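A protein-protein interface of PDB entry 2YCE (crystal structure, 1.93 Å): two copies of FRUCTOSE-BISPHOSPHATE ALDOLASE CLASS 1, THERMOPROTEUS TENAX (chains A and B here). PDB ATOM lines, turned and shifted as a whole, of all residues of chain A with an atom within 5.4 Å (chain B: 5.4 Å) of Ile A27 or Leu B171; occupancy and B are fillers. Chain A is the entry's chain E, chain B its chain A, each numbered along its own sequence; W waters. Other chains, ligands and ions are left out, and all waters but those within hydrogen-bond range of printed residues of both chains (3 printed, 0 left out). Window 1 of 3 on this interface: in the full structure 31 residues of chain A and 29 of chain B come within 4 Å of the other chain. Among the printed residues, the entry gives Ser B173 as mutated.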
ATOM      1  N   ASP A  24     -10.652 -10.711 -23.247  1.00  0.00           N
ATOM      2  CA  ASP A  24     -10.045 -11.101 -21.966  1.00  0.00           C
ATOM      3  C   ASP A  24      -9.428  -9.887 -21.299  1.00  0.00           C
ATOM      4  O   ASP A  24      -8.775 -10.020 -20.278  1.00  0.00           O
ATOM      5  CB  ASP A  24      -8.967 -12.206 -22.139  1.00  0.00           C
ATOM      6  CG  ASP A  24      -7.886 -11.845 -23.170  1.00  0.00           C
ATOM      7  OD1 ASP A  24      -8.212 -11.208 -24.199  1.00  0.00           O
ATOM      8  OD2 ASP A  24      -6.701 -12.229 -22.992  1.00  0.00           O
ATOM      9  N   HIS A  25      -9.660  -8.706 -21.888  1.00  0.00           N
ATOM     10  CA  HIS A  25      -9.052  -7.442 -21.480  1.00  0.00           C
ATOM     11  C   HIS A  25      -9.397  -6.971 -20.062  1.00  0.00           C
ATOM     12  O   HIS A  25      -8.557  -6.369 -19.392  1.00  0.00           O
ATOM     13  CB  HIS A  25      -9.382  -6.358 -22.518  1.00  0.00           C
ATOM     14  CG  HIS A  25      -8.875  -6.678 -23.899  1.00  0.00           C
ATOM     15  ND1 HIS A  25      -9.328  -7.762 -24.633  1.00  0.00           N
ATOM     16  CD2 HIS A  25      -7.967  -6.044 -24.689  1.00  0.00           C
ATOM     17  CE1 HIS A  25      -8.708  -7.791 -25.803  1.00  0.00           C
ATOM     18  NE2 HIS A  25      -7.891  -6.748 -25.869  1.00  0.00           N
ATOM     19  N   GLY A  26     -10.620  -7.268 -19.602  1.00  0.00           N
ATOM     20  CA  GLY A  26     -11.061  -6.910 -18.242  1.00  0.00           C
ATOM     21  C   GLY A  26     -10.099  -7.389 -17.150  1.00  0.00           C
ATOM     22  O   GLY A  26      -9.885  -6.680 -16.174  1.00  0.00           O
ATOM     23  N   ILE A  27      -9.522  -8.577 -17.325  1.00  0.00           N
ATOM     24  CA  ILE A  27      -8.475  -9.068 -16.412  1.00  0.00           C
ATOM     25  C   ILE A  27      -7.059  -8.589 -16.816  1.00  0.00           C
ATOM     26  O   ILE A  27      -6.299  -8.104 -15.972  1.00  0.00           O
ATOM     27  CB  ILE A  27      -8.513 -10.623 -16.132  1.00  0.00           C
ATOM     28  CG1 ILE A  27      -7.464 -11.000 -15.064  1.00  0.00           C
ATOM     29  CG2 ILE A  27      -8.209 -11.476 -17.372  1.00  0.00           C
ATOM     30  CD1 ILE A  27      -7.802 -12.294 -14.205  1.00  0.00           C
ATOM     31  N   GLU A  28      -6.715  -8.733 -18.094  1.00  0.00           N
ATOM     32  CA  GLU A  28      -5.333  -8.420 -18.549  1.00  0.00           C
ATOM     33  C   GLU A  28      -4.945  -6.971 -18.377  1.00  0.00           C
ATOM     34  O   GLU A  28      -3.807  -6.682 -17.945  1.00  0.00           O
ATOM     35  CB  GLU A  28      -5.120  -8.852 -20.000  1.00  0.00           C
ATOM     36  CG  GLU A  28      -5.217 -10.368 -20.188  1.00  0.00           C
ATOM     37  CD  GLU A  28      -4.024 -11.147 -19.591  1.00  0.00           C
ATOM     38  OE1 GLU A  28      -2.867 -10.638 -19.521  1.00  0.00           O
ATOM     39  OE2 GLU A  28      -4.229 -12.316 -19.233  1.00  0.00           O
ATOM     40  N   HIS A  29      -5.861  -6.045 -18.707  1.00  0.00           N
ATOM     41  CA  HIS A  29      -5.557  -4.589 -18.616  1.00  0.00           C
ATOM     42  C   HIS A  29      -6.455  -3.853 -17.657  1.00  0.00           C
ATOM     43  O   HIS A  29      -6.127  -2.750 -17.182  1.00  0.00           O
ATOM     44  CB  HIS A  29      -5.678  -3.916 -19.987  1.00  0.00           C
ATOM     45  CG  HIS A  29      -4.817  -4.552 -21.022  1.00  0.00           C
ATOM     46  ND1 HIS A  29      -5.204  -4.670 -22.340  1.00  0.00           N
ATOM     47  CD2 HIS A  29      -3.607  -5.158 -20.923  1.00  0.00           C
ATOM     48  CE1 HIS A  29      -4.257  -5.298 -23.021  1.00  0.00           C
ATOM     49  NE2 HIS A  29      -3.283  -5.617 -22.184  1.00  0.00           N
ATOM     50  N   GLY A  30      -7.595  -4.468 -17.385  1.00  0.00           N
ATOM     51  CA  GLY A  30      -8.617  -3.868 -16.557  1.00  0.00           C
ATOM     52  C   GLY A  30      -9.461  -2.849 -17.312  1.00  0.00           C
ATOM     53  O   GLY A  30      -9.272  -2.634 -18.506  1.00  0.00           O
ATOM     54  N   GLN A  61     -12.928 -14.987 -20.538  1.00  0.00           N
ATOM     55  CA  GLN A  61     -12.505 -15.688 -19.343  1.00  0.00           C
ATOM     56  C   GLN A  61     -13.737 -16.395 -18.762  1.00  0.00           C
ATOM     57  O   GLN A  61     -14.877 -16.064 -19.122  1.00  0.00           O
ATOM     58  CB  GLN A  61     -11.972 -14.701 -18.288  1.00  0.00           C
ATOM     59  CG  GLN A  61     -10.668 -13.995 -18.661  1.00  0.00           C
ATOM     60  CD  GLN A  61      -9.440 -14.822 -18.303  1.00  0.00           C
ATOM     61  OE1 GLN A  61      -9.486 -15.680 -17.406  1.00  0.00           O
ATOM     62  NE2 GLN A  61      -8.339 -14.574 -19.007  1.00  0.00           N
ATOM     63  N   ARG A  62     -13.501 -17.310 -17.830  1.00  0.00           N
ATOM     64  CA  ARG A  62     -14.587 -18.139 -17.239  1.00  0.00           C
ATOM     65  C   ARG A  62     -15.725 -17.339 -16.600  1.00  0.00           C
ATOM     66  O   ARG A  62     -16.886 -17.727 -16.686  1.00  0.00           O
ATOM     67  CB  ARG A  62     -14.026 -19.117 -16.201  1.00  0.00           C
ATOM     68  CG  ARG A  62     -13.547 -18.380 -14.875  1.00  0.00           C
ATOM     69  CD  ARG A  62     -13.313 -19.363 -13.699  1.00  0.00           C
ATOM     70  NE  ARG A  62     -14.422 -20.316 -13.586  1.00  0.00           N
ATOM     71  CZ  ARG A  62     -14.309 -21.573 -13.171  1.00  0.00           C
ATOM     72  NH1 ARG A  62     -13.118 -22.068 -12.764  1.00  0.00           N
ATOM     73  NH2 ARG A  62     -15.405 -22.328 -13.129  1.00  0.00           N
ATOM     74  N   GLY A  63     -15.417 -16.231 -15.942  1.00  0.00           N
ATOM     75  CA  GLY A  63     -16.500 -15.530 -15.245  1.00  0.00           C
ATOM     76  C   GLY A  63     -17.423 -14.810 -16.215  1.00  0.00           C
ATOM     77  O   GLY A  63     -18.626 -14.767 -16.026  1.00  0.00           O
ATOM     78  N   GLY A  81      -5.103 -15.989 -16.903  1.00  0.00           N
ATOM     79  CA  GLY A  81      -5.041 -14.546 -16.982  1.00  0.00           C
ATOM     80  C   GLY A  81      -4.161 -14.002 -15.876  1.00  0.00           C
ATOM     81  O   GLY A  81      -4.051 -14.596 -14.777  1.00  0.00           O
ATOM     82  N   LYS A  82      -3.527 -12.877 -16.177  1.00  0.00           N
ATOM     83  CA  LYS A  82      -2.768 -12.110 -15.181  1.00  0.00           C
ATOM     84  C   LYS A  82      -3.162 -10.631 -15.318  1.00  0.00           C
ATOM     85  O   LYS A  82      -3.896 -10.266 -16.244  1.00  0.00           O
ATOM     86  CB  LYS A  82      -1.265 -12.276 -15.427  1.00  0.00           C
ATOM     87  CG  LYS A  82      -0.853 -11.728 -16.796  1.00  0.00           C
ATOM     88  CD  LYS A  82       0.667 -11.547 -16.922  1.00  0.00           C
ATOM     89  CE  LYS A  82       1.176 -10.292 -16.205  1.00  0.00           C
ATOM     90  NZ  LYS A  82       1.014  -9.007 -17.051  1.00  0.00           N
ATOM     91  N   THR A  83      -2.640  -9.768 -14.443  1.00  0.00           N
ATOM     92  CA  THR A  83      -2.958  -8.331 -14.533  1.00  0.00           C
ATOM     93  C   THR A  83      -1.716  -7.521 -14.888  1.00  0.00           C
ATOM     94  O   THR A  83      -0.592  -7.994 -14.708  1.00  0.00           O
ATOM     95  CB  THR A  83      -3.500  -7.805 -13.174  1.00  0.00           C
ATOM     96  OG1 THR A  83      -2.420  -7.732 -12.233  1.00  0.00           O
ATOM     97  CG2 THR A  83      -4.625  -8.779 -12.603  1.00  0.00           C
ATOM     98  N   THR A  84      -1.900  -6.272 -15.323  1.00  0.00           N
ATOM     99  CA  THR A  84      -0.754  -5.395 -15.531  1.00  0.00           C
ATOM    100  C   THR A  84      -0.263  -4.797 -14.237  1.00  0.00           C
ATOM    101  O   THR A  84       0.779  -4.138 -14.228  1.00  0.00           O
ATOM    102  CB  THR A  84      -1.083  -4.188 -16.463  1.00  0.00           C
ATOM    103  OG1 THR A  84      -2.269  -3.545 -15.979  1.00  0.00           O
ATOM    104  CG2 THR A  84      -1.296  -4.661 -17.869  1.00  0.00           C
ATOM    105  N   ASN A  95      -7.114 -20.235 -14.428  1.00  0.00           N
ATOM    106  CA  ASN A  95      -8.135 -20.071 -13.350  1.00  0.00           C
ATOM    107  C   ASN A  95      -9.386 -20.951 -13.621  1.00  0.00           C
ATOM    108  O   ASN A  95     -10.443 -20.804 -12.966  1.00  0.00           O
ATOM    109  CB  ASN A  95      -8.556 -18.577 -13.214  1.00  0.00           C
ATOM    110  CG  ASN A  95      -9.021 -18.002 -14.532  1.00  0.00           C
ATOM    111  OD1 ASN A  95     -10.094 -18.381 -15.031  1.00  0.00           O
ATOM    112  ND2 ASN A  95      -8.231 -17.077 -15.114  1.00  0.00           N
ATOM    113  N   ILE B 113      -8.307 -12.129  -2.796  1.00  0.00           N
ATOM    114  CA  ILE B 113      -7.231 -12.071  -3.807  1.00  0.00           C
ATOM    115  C   ILE B 113      -6.518 -10.720  -3.687  1.00  0.00           C
ATOM    116  O   ILE B 113      -7.171  -9.705  -3.372  1.00  0.00           O
ATOM    117  CB  ILE B 113      -7.742 -12.304  -5.271  1.00  0.00           C
ATOM    118  CG1 ILE B 113      -8.885 -11.318  -5.664  1.00  0.00           C
ATOM    119  CG2 ILE B 113      -8.159 -13.808  -5.461  1.00  0.00           C
ATOM    120  CD1 ILE B 113      -9.308 -11.474  -7.163  1.00  0.00           C
ATOM    121  N   PHE B 124      -4.710 -16.975  -7.599  1.00  0.00           N
ATOM    122  CA  PHE B 124      -5.554 -17.288  -8.764  1.00  0.00           C
ATOM    123  C   PHE B 124      -5.672 -18.795  -8.955  1.00  0.00           C
ATOM    124  O   PHE B 124      -6.735 -19.327  -9.275  1.00  0.00           O
ATOM    125  CB  PHE B 124      -5.048 -16.624 -10.075  1.00  0.00           C
ATOM    126  CG  PHE B 124      -5.154 -15.097 -10.090  1.00  0.00           C
ATOM    127  CD1 PHE B 124      -5.895 -14.398  -9.125  1.00  0.00           C
ATOM    128  CD2 PHE B 124      -4.512 -14.360 -11.093  1.00  0.00           C
ATOM    129  CE1 PHE B 124      -5.985 -12.990  -9.149  1.00  0.00           C
ATOM    130  CE2 PHE B 124      -4.587 -12.953 -11.118  1.00  0.00           C
ATOM    131  CZ  PHE B 124      -5.345 -12.265 -10.163  1.00  0.00           C
ATOM    132  N   LEU B 127      -7.904 -20.046  -6.041  1.00  0.00           N
ATOM    133  CA  LEU B 127      -9.309 -19.630  -6.232  1.00  0.00           C
ATOM    134  C   LEU B 127      -9.973 -20.483  -7.303  1.00  0.00           C
ATOM    135  O   LEU B 127     -11.157 -20.760  -7.221  1.00  0.00           O
ATOM    136  CB  LEU B 127      -9.440 -18.136  -6.603  1.00  0.00           C
ATOM    137  CG  LEU B 127     -10.855 -17.566  -6.844  1.00  0.00           C
ATOM    138  CD1 LEU B 127     -11.792 -17.685  -5.594  1.00  0.00           C
ATOM    139  CD2 LEU B 127     -10.826 -16.107  -7.322  1.00  0.00           C
ATOM    140  N   LYS B 131     -13.423 -22.136  -6.649  1.00  0.00           N
ATOM    141  CA  LYS B 131     -14.556 -21.854  -7.512  1.00  0.00           C
ATOM    142  C   LYS B 131     -15.195 -23.159  -8.002  1.00  0.00           C
ATOM    143  O   LYS B 131     -16.433 -23.266  -8.062  1.00  0.00           O
ATOM    144  CB  LYS B 131     -14.119 -20.970  -8.703  1.00  0.00           C
ATOM    145  CG  LYS B 131     -15.116 -20.858  -9.874  1.00  0.00           C
ATOM    146  CD  LYS B 131     -16.417 -20.110  -9.458  1.00  0.00           C
ATOM    147  CE  LYS B 131     -17.454 -20.133 -10.629  1.00  0.00           C
ATOM    148  NZ  LYS B 131     -18.631 -19.258 -10.229  1.00  0.00           N
ATOM    149  N   TYR B 163     -10.627  -1.815 -11.397  1.00  0.00           N
ATOM    150  CA  TYR B 163      -9.878  -3.023 -11.767  1.00  0.00           C
ATOM    151  C   TYR B 163     -10.209  -4.172 -10.801  1.00  0.00           C
ATOM    152  O   TYR B 163     -10.504  -5.300 -11.229  1.00  0.00           O
ATOM    153  CB  TYR B 163      -8.368  -2.739 -11.768  1.00  0.00           C
ATOM    154  CG  TYR B 163      -7.508  -3.545 -12.740  1.00  0.00           C
ATOM    155  CD1 TYR B 163      -7.923  -4.779 -13.247  1.00  0.00           C
ATOM    156  CD2 TYR B 163      -6.230  -3.069 -13.117  1.00  0.00           C
ATOM    157  CE1 TYR B 163      -7.094  -5.513 -14.115  1.00  0.00           C
ATOM    158  CE2 TYR B 163      -5.411  -3.791 -13.979  1.00  0.00           C
ATOM    159  CZ  TYR B 163      -5.840  -5.007 -14.481  1.00  0.00           C
ATOM    160  OH  TYR B 163      -5.009  -5.695 -15.361  1.00  0.00           O
ATOM    161  N   ARG B 166     -13.630  -5.622 -11.672  1.00  0.00           N
ATOM    162  CA  ARG B 166     -13.700  -6.339 -12.948  1.00  0.00           C
ATOM    163  C   ARG B 166     -13.008  -7.703 -12.831  1.00  0.00           C
ATOM    164  O   ARG B 166     -13.524  -8.738 -13.321  1.00  0.00           O
ATOM    165  CB  ARG B 166     -13.069  -5.518 -14.080  1.00  0.00           C
ATOM    166  CG  ARG B 166     -13.193  -6.221 -15.472  1.00  0.00           C
ATOM    167  CD  ARG B 166     -14.662  -6.691 -15.780  1.00  0.00           C
ATOM    168  NE  ARG B 166     -14.800  -7.040 -17.189  1.00  0.00           N
ATOM    169  CZ  ARG B 166     -15.750  -6.602 -18.017  1.00  0.00           C
ATOM    170  NH1 ARG B 166     -16.753  -5.785 -17.595  1.00  0.00           N
ATOM    171  NH2 ARG B 166     -15.703  -6.990 -19.288  1.00  0.00           N
ATOM    172  N   ILE B 167     -11.830  -7.703 -12.214  1.00  0.00           N
ATOM    173  CA  ILE B 167     -11.137  -8.968 -11.919  1.00  0.00           C
ATOM    174  C   ILE B 167     -12.035  -9.996 -11.192  1.00  0.00           C
ATOM    175  O   ILE B 167     -12.049 -11.192 -11.537  1.00  0.00           O
ATOM    176  CB  ILE B 167      -9.857  -8.741 -11.101  1.00  0.00           C
ATOM    177  CG1 ILE B 167      -8.865  -7.885 -11.880  1.00  0.00           C
ATOM    178  CG2 ILE B 167      -9.179 -10.108 -10.694  1.00  0.00           C
ATOM    179  CD1 ILE B 167      -7.766  -7.294 -10.968  1.00  0.00           C
ATOM    180  N   ALA B 168     -12.802  -9.537 -10.213  1.00  0.00           N
ATOM    181  CA  ALA B 168     -13.661 -10.460  -9.461  1.00  0.00           C
ATOM    182  C   ALA B 168     -14.744 -11.040 -10.369  1.00  0.00           C
ATOM    183  O   ALA B 168     -15.106 -12.210 -10.248  1.00  0.00           O
ATOM    184  CB  ALA B 168     -14.292  -9.764  -8.229  1.00  0.00           C
ATOM    185  N   LEU B 169     -15.271 -10.211 -11.267  1.00  0.00           N
ATOM    186  CA  LEU B 169     -16.232 -10.700 -12.246  1.00  0.00           C
ATOM    187  C   LEU B 169     -15.545 -11.725 -13.184  1.00  0.00           C
ATOM    188  O   LEU B 169     -16.066 -12.846 -13.409  1.00  0.00           O
ATOM    189  CB  LEU B 169     -16.812  -9.541 -13.043  1.00  0.00           C
ATOM    190  CG  LEU B 169     -17.562  -9.901 -14.335  1.00  0.00           C
ATOM    191  CD1 LEU B 169     -18.785 -10.773 -14.065  1.00  0.00           C
ATOM    192  CD2 LEU B 169     -17.927  -8.658 -15.172  1.00  0.00           C
ATOM    193  N   GLU B 170     -14.372 -11.365 -13.704  1.00  0.00           N
ATOM    194  CA  GLU B 170     -13.683 -12.213 -14.683  1.00  0.00           C
ATOM    195  C   GLU B 170     -13.392 -13.610 -14.132  1.00  0.00           C
ATOM    196  O   GLU B 170     -13.475 -14.571 -14.875  1.00  0.00           O
ATOM    197  CB  GLU B 170     -12.389 -11.561 -15.166  1.00  0.00           C
ATOM    198  CG  GLU B 170     -12.610 -10.226 -15.886  1.00  0.00           C
ATOM    199  CD  GLU B 170     -12.857 -10.332 -17.388  1.00  0.00           C
ATOM    200  OE1 GLU B 170     -12.496 -11.355 -18.005  1.00  0.00           O
ATOM    201  OE2 GLU B 170     -13.368  -9.340 -17.980  1.00  0.00           O
ATOM    202  N   LEU B 171     -13.053 -13.703 -12.844  1.00  0.00           N
ATOM    203  CA  LEU B 171     -12.573 -14.951 -12.244  1.00  0.00           C
ATOM    204  C   LEU B 171     -13.694 -15.874 -11.745  1.00  0.00           C
ATOM    205  O   LEU B 171     -13.433 -17.021 -11.356  1.00  0.00           O
ATOM    206  CB  LEU B 171     -11.587 -14.666 -11.111  1.00  0.00           C
ATOM    207  CG  LEU B 171     -10.205 -14.078 -11.502  1.00  0.00           C
ATOM    208  CD1 LEU B 171      -9.384 -13.779 -10.226  1.00  0.00           C
ATOM    209  CD2 LEU B 171      -9.396 -15.041 -12.387  1.00  0.00           C
ATOM    210  N   GLY B 172     -14.934 -15.390 -11.762  1.00  0.00           N
ATOM    211  CA  GLY B 172     -16.064 -16.270 -11.441  1.00  0.00           C
ATOM    212  C   GLY B 172     -16.804 -15.979 -10.152  1.00  0.00           C
ATOM    213  O   GLY B 172     -17.653 -16.781  -9.760  1.00  0.00           O
ATOM    214  N   SER B 173     -16.521 -14.852  -9.480  1.00  0.00           N
ATOM    215  CA  SER B 173     -17.234 -14.561  -8.237  1.00  0.00           C
ATOM    216  C   SER B 173     -18.745 -14.457  -8.479  1.00  0.00           C
ATOM    217  O   SER B 173     -19.174 -14.019  -9.540  1.00  0.00           O
ATOM    218  CB  SER B 173     -16.699 -13.280  -7.555  1.00  0.00           C
ATOM    219  OG  SER B 173     -17.145 -12.102  -8.214  1.00  0.00           O
HETATM  220  O   HOH W   1     -11.352 -18.886 -10.629  1.00  0.00           O
HETATM  221  O   HOH W   2     -13.250 -12.256 -20.472  1.00  0.00           O
HETATM  222  O   HOH W   3     -13.110  -8.433 -20.415  1.00  0.00           O
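The side-chain hydroxyl (OH) of Tyr B163 lies within hydrogen-bond range of the backbone carbonyl oxygen (O) of Ile A27, 2.8 Å away. The backbone carbonyl oxygen (O) of Glu A28 is in hydrogen-bond range of the side-chain hydroxyl (OH) of Tyr B163 (3.0 Å). The side-chain hydroxyl of Tyr B163 lies close to the backbone NH of His A29 (3.5 Å). OH of Tyr B163 is in hydrogen-bond range of N of Thr A84 (3.2 Å). N of Gly A63 lies within hydrogen-bond range of O of Glu B170 (2.8 Å).
NZ of Lys B131 sits at hydrogen-bond distance from O of Gly B172 (2.7 Å). O of His A25 is in hydrogen-bond range of N of Gly A30 (2.9 Å). N of Lys A82 lies within hydrogen-bond range of OE2 of Glu A28 (3.2 Å). The backbone carbonyl oxygen (O) of Glu A28 lies close to the backbone NH (N) of Thr A84 (3.3 Å). The side-chain amide nitrogen (ND2) of Asn A95 lies within hydrogen-bond range of the side-chain amide oxygen (OE1) of Gln A61. The guanidinium group of Arg A62 is in hydrogen-bond range of the backbone carbonyl oxygen of Asn A95, at 3.0 Å.
Gly A26 touches Tyr B163 (O to CE1, 3.7 Å). Glu B170 touches Ile A27 (CD to N, 3.8 Å). Leu B171 touches Ile A27. Tyr B163 touches Gly A30 (CE1 to CA, 3.3 Å). CG of Gln A61 touches OE1 of Glu B170, 3.3 Å away. Lys B131 touches Arg A62. CD of Arg A62 touches O of Leu B171, at 3.3 Å. O of Gly A81 touches CD2 of Phe B124 (3.7 Å). Thr A83 touches Tyr B163. Leu B171 touches Asn A95 (CD2 to ND2, 3.6 Å).
Of chain B, only Tyr B163, Glu B170 and Leu B171 come within 4 Å of Ile A27. Leu B171 touches just these residues of chain A: Ile A27 (3.7 Å), Arg A62 (3.3 Å) and Asn A95 (3.6 Å). Of the printed residues of chain A, Ile B167 touches Thr A83. Of the printed residues of chain A, Lys B131 touches Arg A62 (3.5 Å). Asp A24 touches none of the printed residues of chain B. His A25 touches none of the printed residues of chain B. The nearest residue of chain A that does not touch Leu B171 is Gly A63 (4.5 Å).
Of the 13 printed residues of chain B, 9 touch a printed residue of chain A. Hydrophobic or aromatic side chains of chain B within 4 Å of the printed part of chain A: Phe B124, Tyr B163, Ile B167 and Leu B171. Along chain B the printed residues that touch a printed residue of chain A span positions 124 to 172. Printed residues of chain A that touch a printed residue of chain B: Gly A26, Ile A27, Glu A28, His A29, Gly A30, Gln A61, Arg A62, Gly A63, Gly A81, Thr A83, Thr A84 and Asn A95.
No position is printed for both chains. Of the 21 pairs that touch across the chains among the printed residues, none has its exchanged pair printed and touching as well.
Water W3 lies within hydrogen-bond range of the side-chain carboxylate of Glu B170 (2.6 Å), the backbone NH of Gly A26 (2.9 Å) and the guanidinium group of Arg B166 (3.2 Å). Water W2 lies within hydrogen-bond range of the side-chain carboxylate (OE1) of Glu B170 and the backbone NH (N) of Gln A61. Water W1 bridges O of Leu B171 (2.9 Å) and O of Asn A95 (3.2 Å).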
